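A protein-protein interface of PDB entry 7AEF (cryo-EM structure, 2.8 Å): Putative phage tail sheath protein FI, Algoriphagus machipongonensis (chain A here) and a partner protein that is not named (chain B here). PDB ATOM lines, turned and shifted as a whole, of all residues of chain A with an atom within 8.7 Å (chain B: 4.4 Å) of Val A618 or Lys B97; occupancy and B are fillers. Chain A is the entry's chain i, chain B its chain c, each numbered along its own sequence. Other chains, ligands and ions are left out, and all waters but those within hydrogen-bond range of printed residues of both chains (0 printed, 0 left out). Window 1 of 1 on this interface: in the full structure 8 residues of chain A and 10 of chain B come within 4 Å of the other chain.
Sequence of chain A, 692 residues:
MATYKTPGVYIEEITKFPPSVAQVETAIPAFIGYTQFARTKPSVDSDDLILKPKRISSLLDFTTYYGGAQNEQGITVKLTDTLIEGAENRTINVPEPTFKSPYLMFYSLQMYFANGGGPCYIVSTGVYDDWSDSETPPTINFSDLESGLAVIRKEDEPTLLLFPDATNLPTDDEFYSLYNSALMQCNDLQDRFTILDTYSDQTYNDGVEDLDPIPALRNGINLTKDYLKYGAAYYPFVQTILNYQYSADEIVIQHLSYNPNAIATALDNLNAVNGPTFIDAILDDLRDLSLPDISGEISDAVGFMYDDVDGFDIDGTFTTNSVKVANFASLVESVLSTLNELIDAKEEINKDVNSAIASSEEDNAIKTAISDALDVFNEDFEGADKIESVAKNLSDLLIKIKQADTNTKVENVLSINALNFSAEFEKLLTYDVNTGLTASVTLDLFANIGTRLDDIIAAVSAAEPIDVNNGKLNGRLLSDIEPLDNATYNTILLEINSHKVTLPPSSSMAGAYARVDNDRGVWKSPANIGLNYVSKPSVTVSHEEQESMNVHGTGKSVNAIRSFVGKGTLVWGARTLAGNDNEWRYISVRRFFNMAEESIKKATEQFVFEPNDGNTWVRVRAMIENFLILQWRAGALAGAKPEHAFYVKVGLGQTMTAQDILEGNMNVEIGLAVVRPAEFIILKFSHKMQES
Pro B105 touches Asn A615 (CD to OD1, 2.8 Å).
CE of Lys B97 touches CG1 of Val A618 (3.9 Å).
Val A618 touches Thr B108 (CG2 to OG1, 3.8 Å).
Arg A619 touches Lys B97 (CG to NZ, 3.8 Å).
NZ of Lys B97 is in salt-bridge range of OE1 of Glu B15, 3.9 Å away.
The backbone carbonyl oxygen (O) of Leu B13 sits at hydrogen-bond distance from the backbone NH (N) of Lys B97 (3.0 Å).
The backbone carbonyl oxygen (O) of Glu B15 lies within hydrogen-bond range of the backbone NH (N) of Thr B95.
Of the 21 printed residues of chain A, 3 touch a printed residue of chain B.
Printed residues of chain A that touch a printed residue of chain B: Asn A615, Val A618 and Arg A619.
Printed residues of chain B that touch a printed residue of chain A: Glu B15, Lys B97, Pro B105 and Thr B108.
Hydrophobic or aromatic side chains of chain B within 4 Å of the printed part of chain A: Pro B105.
Among the printed residues, Asp or Glu carboxylates within 4 Å of a Lys or Arg side-chain nitrogen of the other chain: Arg A619 with Glu B15.
Of the printed residues of chain B, Val A618 touches Lys B97 and Thr B108.
Lys B97 touches just these residues of chain A: Asn A615, Val A618 and Arg A619.
Of the printed residues of chain A, Glu B15 touches Arg A619.
Of the printed residues of chain B, Asn A615 touches Lys B97 (2.9 Å) and Pro B105 (2.8 Å).
Of the printed residues of chain A, Pro B105 touches Asn A615 (2.8 Å).
Of the printed residues of chain B, Arg A619 touches Glu B15 and Lys B97.
Thr B95 touches none of the printed residues of chain A.
Pro A611 touches none of the printed residues of chain B.
OE1 of Glu B15 is in salt-bridge range of NE of Arg A619 (3.8 Å).
O of Asn A615 sits at hydrogen-bond distance from NZ of Lys B97 (2.9 Å).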
ATOM      1  N   PHE A 607      -9.056  29.652  22.481  1.00  0.00           N
ATOM      2  CA  PHE A 607      -9.623  28.579  23.284  1.00  0.00           C
ATOM      3  C   PHE A 607      -9.279  28.667  24.766  1.00  0.00           C
ATOM      4  O   PHE A 607      -9.638  27.768  25.525  1.00  0.00           O
ATOM      5  CB  PHE A 607      -9.138  27.230  22.786  1.00  0.00           C
ATOM      6  CG  PHE A 607      -9.511  26.925  21.398  1.00  0.00           C
ATOM      7  CD1 PHE A 607      -8.582  27.051  20.401  1.00  0.00           C
ATOM      8  CD2 PHE A 607     -10.773  26.499  21.075  1.00  0.00           C
ATOM      9  CE1 PHE A 607      -8.899  26.763  19.117  1.00  0.00           C
ATOM     10  CE2 PHE A 607     -11.090  26.213  19.778  1.00  0.00           C
ATOM     11  CZ  PHE A 607     -10.147  26.348  18.800  1.00  0.00           C
ATOM     12  N   GLU A 610     -12.257  28.279  27.276  1.00  0.00           N
ATOM     13  CA  GLU A 610     -13.271  27.315  26.888  1.00  0.00           C
ATOM     14  C   GLU A 610     -13.288  26.149  27.885  1.00  0.00           C
ATOM     15  O   GLU A 610     -12.314  25.948  28.599  1.00  0.00           O
ATOM     16  CB  GLU A 610     -12.995  26.831  25.464  1.00  0.00           C
ATOM     17  CG  GLU A 610     -13.173  27.902  24.436  1.00  0.00           C
ATOM     18  CD  GLU A 610     -14.598  28.284  24.266  1.00  0.00           C
ATOM     19  OE1 GLU A 610     -15.382  27.431  23.885  1.00  0.00           O
ATOM     20  OE2 GLU A 610     -14.938  29.420  24.534  1.00  0.00           O
ATOM     21  N   PRO A 611     -14.404  25.408  27.988  1.00  0.00           N
ATOM     22  CA  PRO A 611     -14.497  24.190  28.807  1.00  0.00           C
ATOM     23  C   PRO A 611     -13.445  23.181  28.391  1.00  0.00           C
ATOM     24  O   PRO A 611     -13.123  23.067  27.205  1.00  0.00           O
ATOM     25  CB  PRO A 611     -15.908  23.681  28.488  1.00  0.00           C
ATOM     26  CG  PRO A 611     -16.670  24.914  28.078  1.00  0.00           C
ATOM     27  CD  PRO A 611     -15.681  25.780  27.360  1.00  0.00           C
ATOM     28  N   ASP A 613     -12.906  19.758  27.715  1.00  0.00           N
ATOM     29  CA  ASP A 613     -13.620  18.526  27.401  1.00  0.00           C
ATOM     30  C   ASP A 613     -13.422  18.208  25.909  1.00  0.00           C
ATOM     31  O   ASP A 613     -12.867  19.011  25.157  1.00  0.00           O
ATOM     32  CB  ASP A 613     -15.106  18.721  27.738  1.00  0.00           C
ATOM     33  CG  ASP A 613     -15.876  17.423  27.965  1.00  0.00           C
ATOM     34  OD1 ASP A 613     -15.456  16.375  27.498  1.00  0.00           O
ATOM     35  OD2 ASP A 613     -16.909  17.482  28.615  1.00  0.00           O
ATOM     36  N   GLY A 614     -14.002  17.083  25.475  1.00  0.00           N
ATOM     37  CA  GLY A 614     -13.868  16.575  24.113  1.00  0.00           C
ATOM     38  C   GLY A 614     -14.287  17.530  23.008  1.00  0.00           C
ATOM     39  O   GLY A 614     -13.693  17.526  21.928  1.00  0.00           O
ATOM     40  N   ASN A 615     -15.266  18.393  23.275  1.00  0.00           N
ATOM     41  CA  ASN A 615     -15.740  19.330  22.263  1.00  0.00           C
ATOM     42  C   ASN A 615     -14.772  20.468  21.999  1.00  0.00           C
ATOM     43  O   ASN A 615     -14.945  21.211  21.027  1.00  0.00           O
ATOM     44  CB  ASN A 615     -17.082  19.897  22.665  1.00  0.00           C
ATOM     45  CG  ASN A 615     -18.180  18.903  22.549  1.00  0.00           C
ATOM     46  OD1 ASN A 615     -18.110  17.944  21.782  1.00  0.00           O
ATOM     47  ND2 ASN A 615     -19.213  19.113  23.312  1.00  0.00           N
ATOM     48  N   THR A 616     -13.765  20.619  22.841  1.00  0.00           N
ATOM     49  CA  THR A 616     -12.752  21.631  22.665  1.00  0.00           C
ATOM     50  C   THR A 616     -11.518  20.970  22.118  1.00  0.00           C
ATOM     51  O   THR A 616     -10.922  21.459  21.162  1.00  0.00           O
ATOM     52  CB  THR A 616     -12.430  22.346  23.991  1.00  0.00           C
ATOM     53  OG1 THR A 616     -13.625  22.924  24.535  1.00  0.00           O
ATOM     54  CG2 THR A 616     -11.406  23.460  23.751  1.00  0.00           C
ATOM     55  N   TRP A 617     -11.186  19.802  22.658  1.00  0.00           N
ATOM     56  CA  TRP A 617      -9.971  19.110  22.257  1.00  0.00           C
ATOM     57  C   TRP A 617      -9.950  18.875  20.752  1.00  0.00           C
ATOM     58  O   TRP A 617      -8.947  19.144  20.081  1.00  0.00           O
ATOM     59  CB  TRP A 617      -9.879  17.781  23.004  1.00  0.00           C
ATOM     60  CG  TRP A 617      -9.872  17.944  24.494  1.00  0.00           C
ATOM     61  CD1 TRP A 617      -9.643  19.079  25.179  1.00  0.00           C
ATOM     62  CD2 TRP A 617     -10.130  16.952  25.477  1.00  0.00           C
ATOM     63  NE1 TRP A 617      -9.746  18.867  26.494  1.00  0.00           N
ATOM     64  CE2 TRP A 617     -10.051  17.571  26.707  1.00  0.00           C
ATOM     65  CE3 TRP A 617     -10.428  15.604  25.430  1.00  0.00           C
ATOM     66  CZ2 TRP A 617     -10.262  16.919  27.872  1.00  0.00           C
ATOM     67  CZ3 TRP A 617     -10.638  14.937  26.614  1.00  0.00           C
ATOM     68  CH2 TRP A 617     -10.558  15.592  27.808  1.00  0.00           C
ATOM     69  N   VAL A 618     -11.097  18.491  20.204  1.00  0.00           N
ATOM     70  CA  VAL A 618     -11.244  18.252  18.776  1.00  0.00           C
ATOM     71  C   VAL A 618     -11.083  19.513  17.922  1.00  0.00           C
ATOM     72  O   VAL A 618     -10.630  19.427  16.773  1.00  0.00           O
ATOM     73  CB  VAL A 618     -12.601  17.578  18.513  1.00  0.00           C
ATOM     74  CG1 VAL A 618     -13.768  18.548  18.723  1.00  0.00           C
ATOM     75  CG2 VAL A 618     -12.621  17.002  17.121  1.00  0.00           C
ATOM     76  N   ARG A 619     -11.560  20.657  18.410  1.00  0.00           N
ATOM     77  CA  ARG A 619     -11.433  21.908  17.693  1.00  0.00           C
ATOM     78  C   ARG A 619      -9.999  22.400  17.656  1.00  0.00           C
ATOM     79  O   ARG A 619      -9.580  22.945  16.644  1.00  0.00           O
ATOM     80  CB  ARG A 619     -12.384  22.955  18.262  1.00  0.00           C
ATOM     81  CG  ARG A 619     -13.822  22.492  18.234  1.00  0.00           C
ATOM     82  CD  ARG A 619     -14.731  23.551  17.665  1.00  0.00           C
ATOM     83  NE  ARG A 619     -14.947  24.633  18.613  1.00  0.00           N
ATOM     84  CZ  ARG A 619     -15.150  25.897  18.276  1.00  0.00           C
ATOM     85  NH1 ARG A 619     -15.149  26.271  17.004  1.00  0.00           N
ATOM     86  NH2 ARG A 619     -15.328  26.795  19.224  1.00  0.00           N
ATOM     87  N   VAL A 620      -9.256  22.217  18.748  1.00  0.00           N
ATOM     88  CA  VAL A 620      -7.857  22.599  18.828  1.00  0.00           C
ATOM     89  C   VAL A 620      -7.053  21.779  17.845  1.00  0.00           C
ATOM     90  O   VAL A 620      -6.236  22.322  17.098  1.00  0.00           O
ATOM     91  CB  VAL A 620      -7.343  22.435  20.271  1.00  0.00           C
ATOM     92  CG1 VAL A 620      -5.833  22.617  20.340  1.00  0.00           C
ATOM     93  CG2 VAL A 620      -8.026  23.463  21.149  1.00  0.00           C
ATOM     94  N   ARG A 621      -7.303  20.468  17.801  1.00  0.00           N
ATOM     95  CA  ARG A 621      -6.599  19.636  16.837  1.00  0.00           C
ATOM     96  C   ARG A 621      -6.852  20.041  15.401  1.00  0.00           C
ATOM     97  O   ARG A 621      -5.899  20.156  14.630  1.00  0.00           O
ATOM     98  CB  ARG A 621      -6.993  18.188  16.938  1.00  0.00           C
ATOM     99  CG  ARG A 621      -6.420  17.427  18.062  1.00  0.00           C
ATOM    100  CD  ARG A 621      -6.872  16.023  17.994  1.00  0.00           C
ATOM    101  NE  ARG A 621      -6.505  15.433  16.704  1.00  0.00           N
ATOM    102  CZ  ARG A 621      -6.895  14.240  16.248  1.00  0.00           C
ATOM    103  NH1 ARG A 621      -7.653  13.446  16.989  1.00  0.00           N
ATOM    104  NH2 ARG A 621      -6.523  13.862  15.033  1.00  0.00           N
ATOM    105  N   ALA A 622      -8.110  20.265  15.025  1.00  0.00           N
ATOM    106  CA  ALA A 622      -8.386  20.578  13.632  1.00  0.00           C
ATOM    107  C   ALA A 622      -7.653  21.825  13.178  1.00  0.00           C
ATOM    108  O   ALA A 622      -7.059  21.848  12.098  1.00  0.00           O
ATOM    109  CB  ALA A 622      -9.873  20.774  13.443  1.00  0.00           C
ATOM    110  N   MET A 623      -7.624  22.831  14.032  1.00  0.00           N
ATOM    111  CA  MET A 623      -6.960  24.072  13.702  1.00  0.00           C
ATOM    112  C   MET A 623      -5.456  23.920  13.518  1.00  0.00           C
ATOM    113  O   MET A 623      -4.886  24.466  12.564  1.00  0.00           O
ATOM    114  CB  MET A 623      -7.244  25.057  14.788  1.00  0.00           C
ATOM    115  CG  MET A 623      -6.587  26.356  14.576  1.00  0.00           C
ATOM    116  SD  MET A 623      -6.808  27.363  15.952  1.00  0.00           S
ATOM    117  CE  MET A 623      -5.673  26.580  17.088  1.00  0.00           C
ATOM    118  N   ILE A 624      -4.800  23.201  14.428  1.00  0.00           N
ATOM    119  CA  ILE A 624      -3.361  23.028  14.326  1.00  0.00           C
ATOM    120  C   ILE A 624      -3.013  22.275  13.060  1.00  0.00           C
ATOM    121  O   ILE A 624      -2.049  22.626  12.370  1.00  0.00           O
ATOM    122  CB  ILE A 624      -2.781  22.313  15.553  1.00  0.00           C
ATOM    123  CG1 ILE A 624      -2.944  23.211  16.774  1.00  0.00           C
ATOM    124  CG2 ILE A 624      -1.278  22.010  15.309  1.00  0.00           C
ATOM    125  CD1 ILE A 624      -2.707  22.531  18.081  1.00  0.00           C
ATOM    126  N   GLU A 625      -3.773  21.221  12.753  1.00  0.00           N
ATOM    127  CA  GLU A 625      -3.525  20.442  11.553  1.00  0.00           C
ATOM    128  C   GLU A 625      -3.659  21.293  10.296  1.00  0.00           C
ATOM    129  O   GLU A 625      -2.852  21.150   9.378  1.00  0.00           O
ATOM    130  CB  GLU A 625      -4.475  19.252  11.493  1.00  0.00           C
ATOM    131  CG  GLU A 625      -4.203  18.159  12.529  1.00  0.00           C
ATOM    132  CD  GLU A 625      -5.272  17.089  12.542  1.00  0.00           C
ATOM    133  OE1 GLU A 625      -6.248  17.245  11.833  1.00  0.00           O
ATOM    134  OE2 GLU A 625      -5.125  16.101  13.258  1.00  0.00           O
ATOM    135  N   VAL A 648      -0.458  15.523  15.603  1.00  0.00           N
ATOM    136  CA  VAL A 648      -0.966  16.238  16.775  1.00  0.00           C
ATOM    137  C   VAL A 648      -1.758  15.271  17.661  1.00  0.00           C
ATOM    138  O   VAL A 648      -2.667  14.609  17.166  1.00  0.00           O
ATOM    139  CB  VAL A 648      -1.880  17.406  16.347  1.00  0.00           C
ATOM    140  CG1 VAL A 648      -2.387  18.167  17.569  1.00  0.00           C
ATOM    141  CG2 VAL A 648      -1.154  18.347  15.382  1.00  0.00           C
ATOM    142  N   VAL A 650      -4.066  14.921  21.299  1.00  0.00           N
ATOM    143  CA  VAL A 650      -4.732  15.568  22.429  1.00  0.00           C
ATOM    144  C   VAL A 650      -5.736  14.616  23.055  1.00  0.00           C
ATOM    145  O   VAL A 650      -6.608  14.122  22.345  1.00  0.00           O
ATOM    146  CB  VAL A 650      -5.503  16.822  21.977  1.00  0.00           C
ATOM    147  CG1 VAL A 650      -6.142  17.513  23.167  1.00  0.00           C
ATOM    148  CG2 VAL A 650      -4.614  17.761  21.254  1.00  0.00           C
ATOM    149  N   GLY A 651      -5.714  14.428  24.366  1.00  0.00           N
ATOM    150  CA  GLY A 651      -6.790  13.632  24.939  1.00  0.00           C
ATOM    151  C   GLY A 651      -6.506  13.067  26.313  1.00  0.00           C
ATOM    152  O   GLY A 651      -5.364  12.931  26.757  1.00  0.00           O
ATOM    153  N   MET A 656      -3.273  13.728  28.792  1.00  0.00           N
ATOM    154  CA  MET A 656      -3.802  14.272  30.041  1.00  0.00           C
ATOM    155  C   MET A 656      -4.308  13.225  31.024  1.00  0.00           C
ATOM    156  O   MET A 656      -4.758  12.135  30.645  1.00  0.00           O
ATOM    157  CB  MET A 656      -4.967  15.215  29.763  1.00  0.00           C
ATOM    158  CG  MET A 656      -4.610  16.446  29.017  1.00  0.00           C
ATOM    159  SD  MET A 656      -6.036  17.431  28.522  1.00  0.00           S
ATOM    160  CE  MET A 656      -6.601  16.602  27.070  1.00  0.00           C
ATOM    161  N   MET A 666      -4.267  21.678  29.915  1.00  0.00           N
ATOM    162  CA  MET A 666      -4.536  20.964  28.676  1.00  0.00           C
ATOM    163  C   MET A 666      -3.218  20.706  27.966  1.00  0.00           C
ATOM    164  O   MET A 666      -2.462  21.637  27.695  1.00  0.00           O
ATOM    165  CB  MET A 666      -5.506  21.751  27.799  1.00  0.00           C
ATOM    166  CG  MET A 666      -5.822  21.097  26.482  1.00  0.00           C
ATOM    167  SD  MET A 666      -7.049  21.983  25.539  1.00  0.00           S
ATOM    168  CE  MET A 666      -6.926  21.058  24.045  1.00  0.00           C
ATOM    169  N   PHE B  12     -26.755  16.750  16.574  1.00  0.00           N
ATOM    170  CA  PHE B  12     -25.547  17.297  15.955  1.00  0.00           C
ATOM    171  C   PHE B  12     -25.356  18.796  16.234  1.00  0.00           C
ATOM    172  O   PHE B  12     -26.303  19.504  16.570  1.00  0.00           O
ATOM    173  CB  PHE B  12     -25.591  17.060  14.439  1.00  0.00           C
ATOM    174  CG  PHE B  12     -26.814  17.649  13.765  1.00  0.00           C
ATOM    175  CD1 PHE B  12     -26.820  18.944  13.275  1.00  0.00           C
ATOM    176  CD2 PHE B  12     -27.964  16.900  13.620  1.00  0.00           C
ATOM    177  CE1 PHE B  12     -27.956  19.472  12.694  1.00  0.00           C
ATOM    178  CE2 PHE B  12     -29.084  17.428  13.024  1.00  0.00           C
ATOM    179  CZ  PHE B  12     -29.073  18.715  12.554  1.00  0.00           C
ATOM    180  N   LEU B  13     -24.133  19.293  15.978  1.00  0.00           N
ATOM    181  CA  LEU B  13     -23.726  20.681  16.240  1.00  0.00           C
ATOM    182  C   LEU B  13     -22.911  21.304  15.091  1.00  0.00           C
ATOM    183  O   LEU B  13     -22.013  20.648  14.575  1.00  0.00           O
ATOM    184  CB  LEU B  13     -22.856  20.677  17.491  1.00  0.00           C
ATOM    185  CG  LEU B  13     -22.369  21.789  18.314  1.00  0.00           C
ATOM    186  CD1 LEU B  13     -23.293  22.861  18.546  1.00  0.00           C
ATOM    187  CD2 LEU B  13     -21.633  21.323  19.460  1.00  0.00           C
ATOM    188  N   GLU B  15     -20.261  24.407  14.163  1.00  0.00           N
ATOM    189  CA  GLU B  15     -19.462  25.501  14.716  1.00  0.00           C
ATOM    190  C   GLU B  15     -18.605  26.177  13.659  1.00  0.00           C
ATOM    191  O   GLU B  15     -18.095  25.542  12.746  1.00  0.00           O
ATOM    192  CB  GLU B  15     -18.528  25.056  15.878  1.00  0.00           C
ATOM    193  CG  GLU B  15     -19.322  24.370  16.935  1.00  0.00           C
ATOM    194  CD  GLU B  15     -19.146  24.951  18.287  1.00  0.00           C
ATOM    195  OE1 GLU B  15     -18.709  24.299  19.247  1.00  0.00           O
ATOM    196  OE2 GLU B  15     -19.301  26.188  18.307  1.00  0.00           O
ATOM    197  N   THR B  95     -16.744  23.189  11.561  1.00  0.00           N
ATOM    198  CA  THR B  95     -16.781  21.835  12.097  1.00  0.00           C
ATOM    199  C   THR B  95     -18.189  21.304  12.214  1.00  0.00           C
ATOM    200  O   THR B  95     -19.061  21.972  12.765  1.00  0.00           O
ATOM    201  CB  THR B  95     -16.034  21.695  13.442  1.00  0.00           C
ATOM    202  OG1 THR B  95     -14.711  22.226  13.351  1.00  0.00           O
ATOM    203  CG2 THR B  95     -16.030  20.283  13.945  1.00  0.00           C
ATOM    204  N   VAL B  96     -18.423  20.108  11.687  1.00  0.00           N
ATOM    205  CA  VAL B  96     -19.714  19.448  11.829  1.00  0.00           C
ATOM    206  C   VAL B  96     -19.533  18.298  12.801  1.00  0.00           C
ATOM    207  O   VAL B  96     -18.675  17.444  12.590  1.00  0.00           O
ATOM    208  CB  VAL B  96     -20.260  18.926  10.487  1.00  0.00           C
ATOM    209  CG1 VAL B  96     -21.522  18.105  10.707  1.00  0.00           C
ATOM    210  CG2 VAL B  96     -20.526  20.080   9.534  1.00  0.00           C
ATOM    211  N   LYS B  97     -20.337  18.255  13.854  1.00  0.00           N
ATOM    212  CA  LYS B  97     -20.180  17.220  14.871  1.00  0.00           C
ATOM    213  C   LYS B  97     -21.413  16.343  15.004  1.00  0.00           C
ATOM    214  O   LYS B  97     -22.500  16.849  15.245  1.00  0.00           O
ATOM    215  CB  LYS B  97     -19.905  17.840  16.236  1.00  0.00           C
ATOM    216  CG  LYS B  97     -18.647  18.663  16.339  1.00  0.00           C
ATOM    217  CD  LYS B  97     -18.513  19.296  17.711  1.00  0.00           C
ATOM    218  CE  LYS B  97     -17.204  20.050  17.850  1.00  0.00           C
ATOM    219  NZ  LYS B  97     -17.095  20.783  19.145  1.00  0.00           N
ATOM    220  N   LEU B  98     -21.234  15.031  14.933  1.00  0.00           N
ATOM    221  CA  LEU B  98     -22.303  14.076  15.199  1.00  0.00           C
ATOM    222  C   LEU B  98     -22.115  13.604  16.639  1.00  0.00           C
ATOM    223  O   LEU B  98     -21.034  13.129  16.982  1.00  0.00           O
ATOM    224  CB  LEU B  98     -22.242  12.916  14.203  1.00  0.00           C
ATOM    225  CG  LEU B  98     -23.281  11.801  14.313  1.00  0.00           C
ATOM    226  CD1 LEU B  98     -24.679  12.323  13.982  1.00  0.00           C
ATOM    227  CD2 LEU B  98     -22.890  10.667  13.387  1.00  0.00           C
ATOM    228  N   LEU B  99     -23.134  13.756  17.489  1.00  0.00           N
ATOM    229  CA  LEU B  99     -22.973  13.543  18.931  1.00  0.00           C
ATOM    230  C   LEU B  99     -23.548  12.249  19.515  1.00  0.00           C
ATOM    231  O   LEU B  99     -24.542  11.704  19.033  1.00  0.00           O
ATOM    232  CB  LEU B  99     -23.616  14.685  19.692  1.00  0.00           C
ATOM    233  CG  LEU B  99     -23.141  16.098  19.427  1.00  0.00           C
ATOM    234  CD1 LEU B  99     -23.997  16.999  20.253  1.00  0.00           C
ATOM    235  CD2 LEU B  99     -21.679  16.262  19.775  1.00  0.00           C
ATOM    236  N   PRO B 105     -18.684  14.225  20.751  1.00  0.00           N
ATOM    237  CA  PRO B 105     -18.622  13.737  19.359  1.00  0.00           C
ATOM    238  C   PRO B 105     -18.387  12.242  19.189  1.00  0.00           C
ATOM    239  O   PRO B 105     -17.454  11.681  19.756  1.00  0.00           O
ATOM    240  CB  PRO B 105     -17.423  14.497  18.802  1.00  0.00           C
ATOM    241  CG  PRO B 105     -17.277  15.688  19.679  1.00  0.00           C
ATOM    242  CD  PRO B 105     -17.680  15.261  21.023  1.00  0.00           C
ATOM    243  N   MET B 107     -18.155  11.391  15.862  1.00  0.00           N
ATOM    244  CA  MET B 107     -17.388  11.629  14.656  1.00  0.00           C
ATOM    245  C   MET B 107     -17.523  13.076  14.199  1.00  0.00           C
ATOM    246  O   MET B 107     -18.604  13.665  14.312  1.00  0.00           O
ATOM    247  CB  MET B 107     -17.873  10.703  13.551  1.00  0.00           C
ATOM    248  CG  MET B 107     -17.257  10.956  12.218  1.00  0.00           C
ATOM    249  SD  MET B 107     -17.698   9.744  11.024  1.00  0.00           S
ATOM    250  CE  MET B 107     -16.647  10.328   9.727  1.00  0.00           C
ATOM    251  N   THR B 108     -16.430  13.657  13.664  1.00  0.00           N
ATOM    252  CA  THR B 108     -16.555  15.015  13.165  1.00  0.00           C
ATOM    253  C   THR B 108     -16.008  15.152  11.739  1.00  0.00           C
ATOM    254  O   THR B 108     -15.183  14.364  11.263  1.00  0.00           O
ATOM    255  CB  THR B 108     -15.785  16.040  13.996  1.00  0.00           C
ATOM    256  OG1 THR B 108     -14.400  15.728  14.002  1.00  0.00           O
ATOM    257  CG2 THR B 108     -16.213  15.891  15.460  1.00  0.00           C
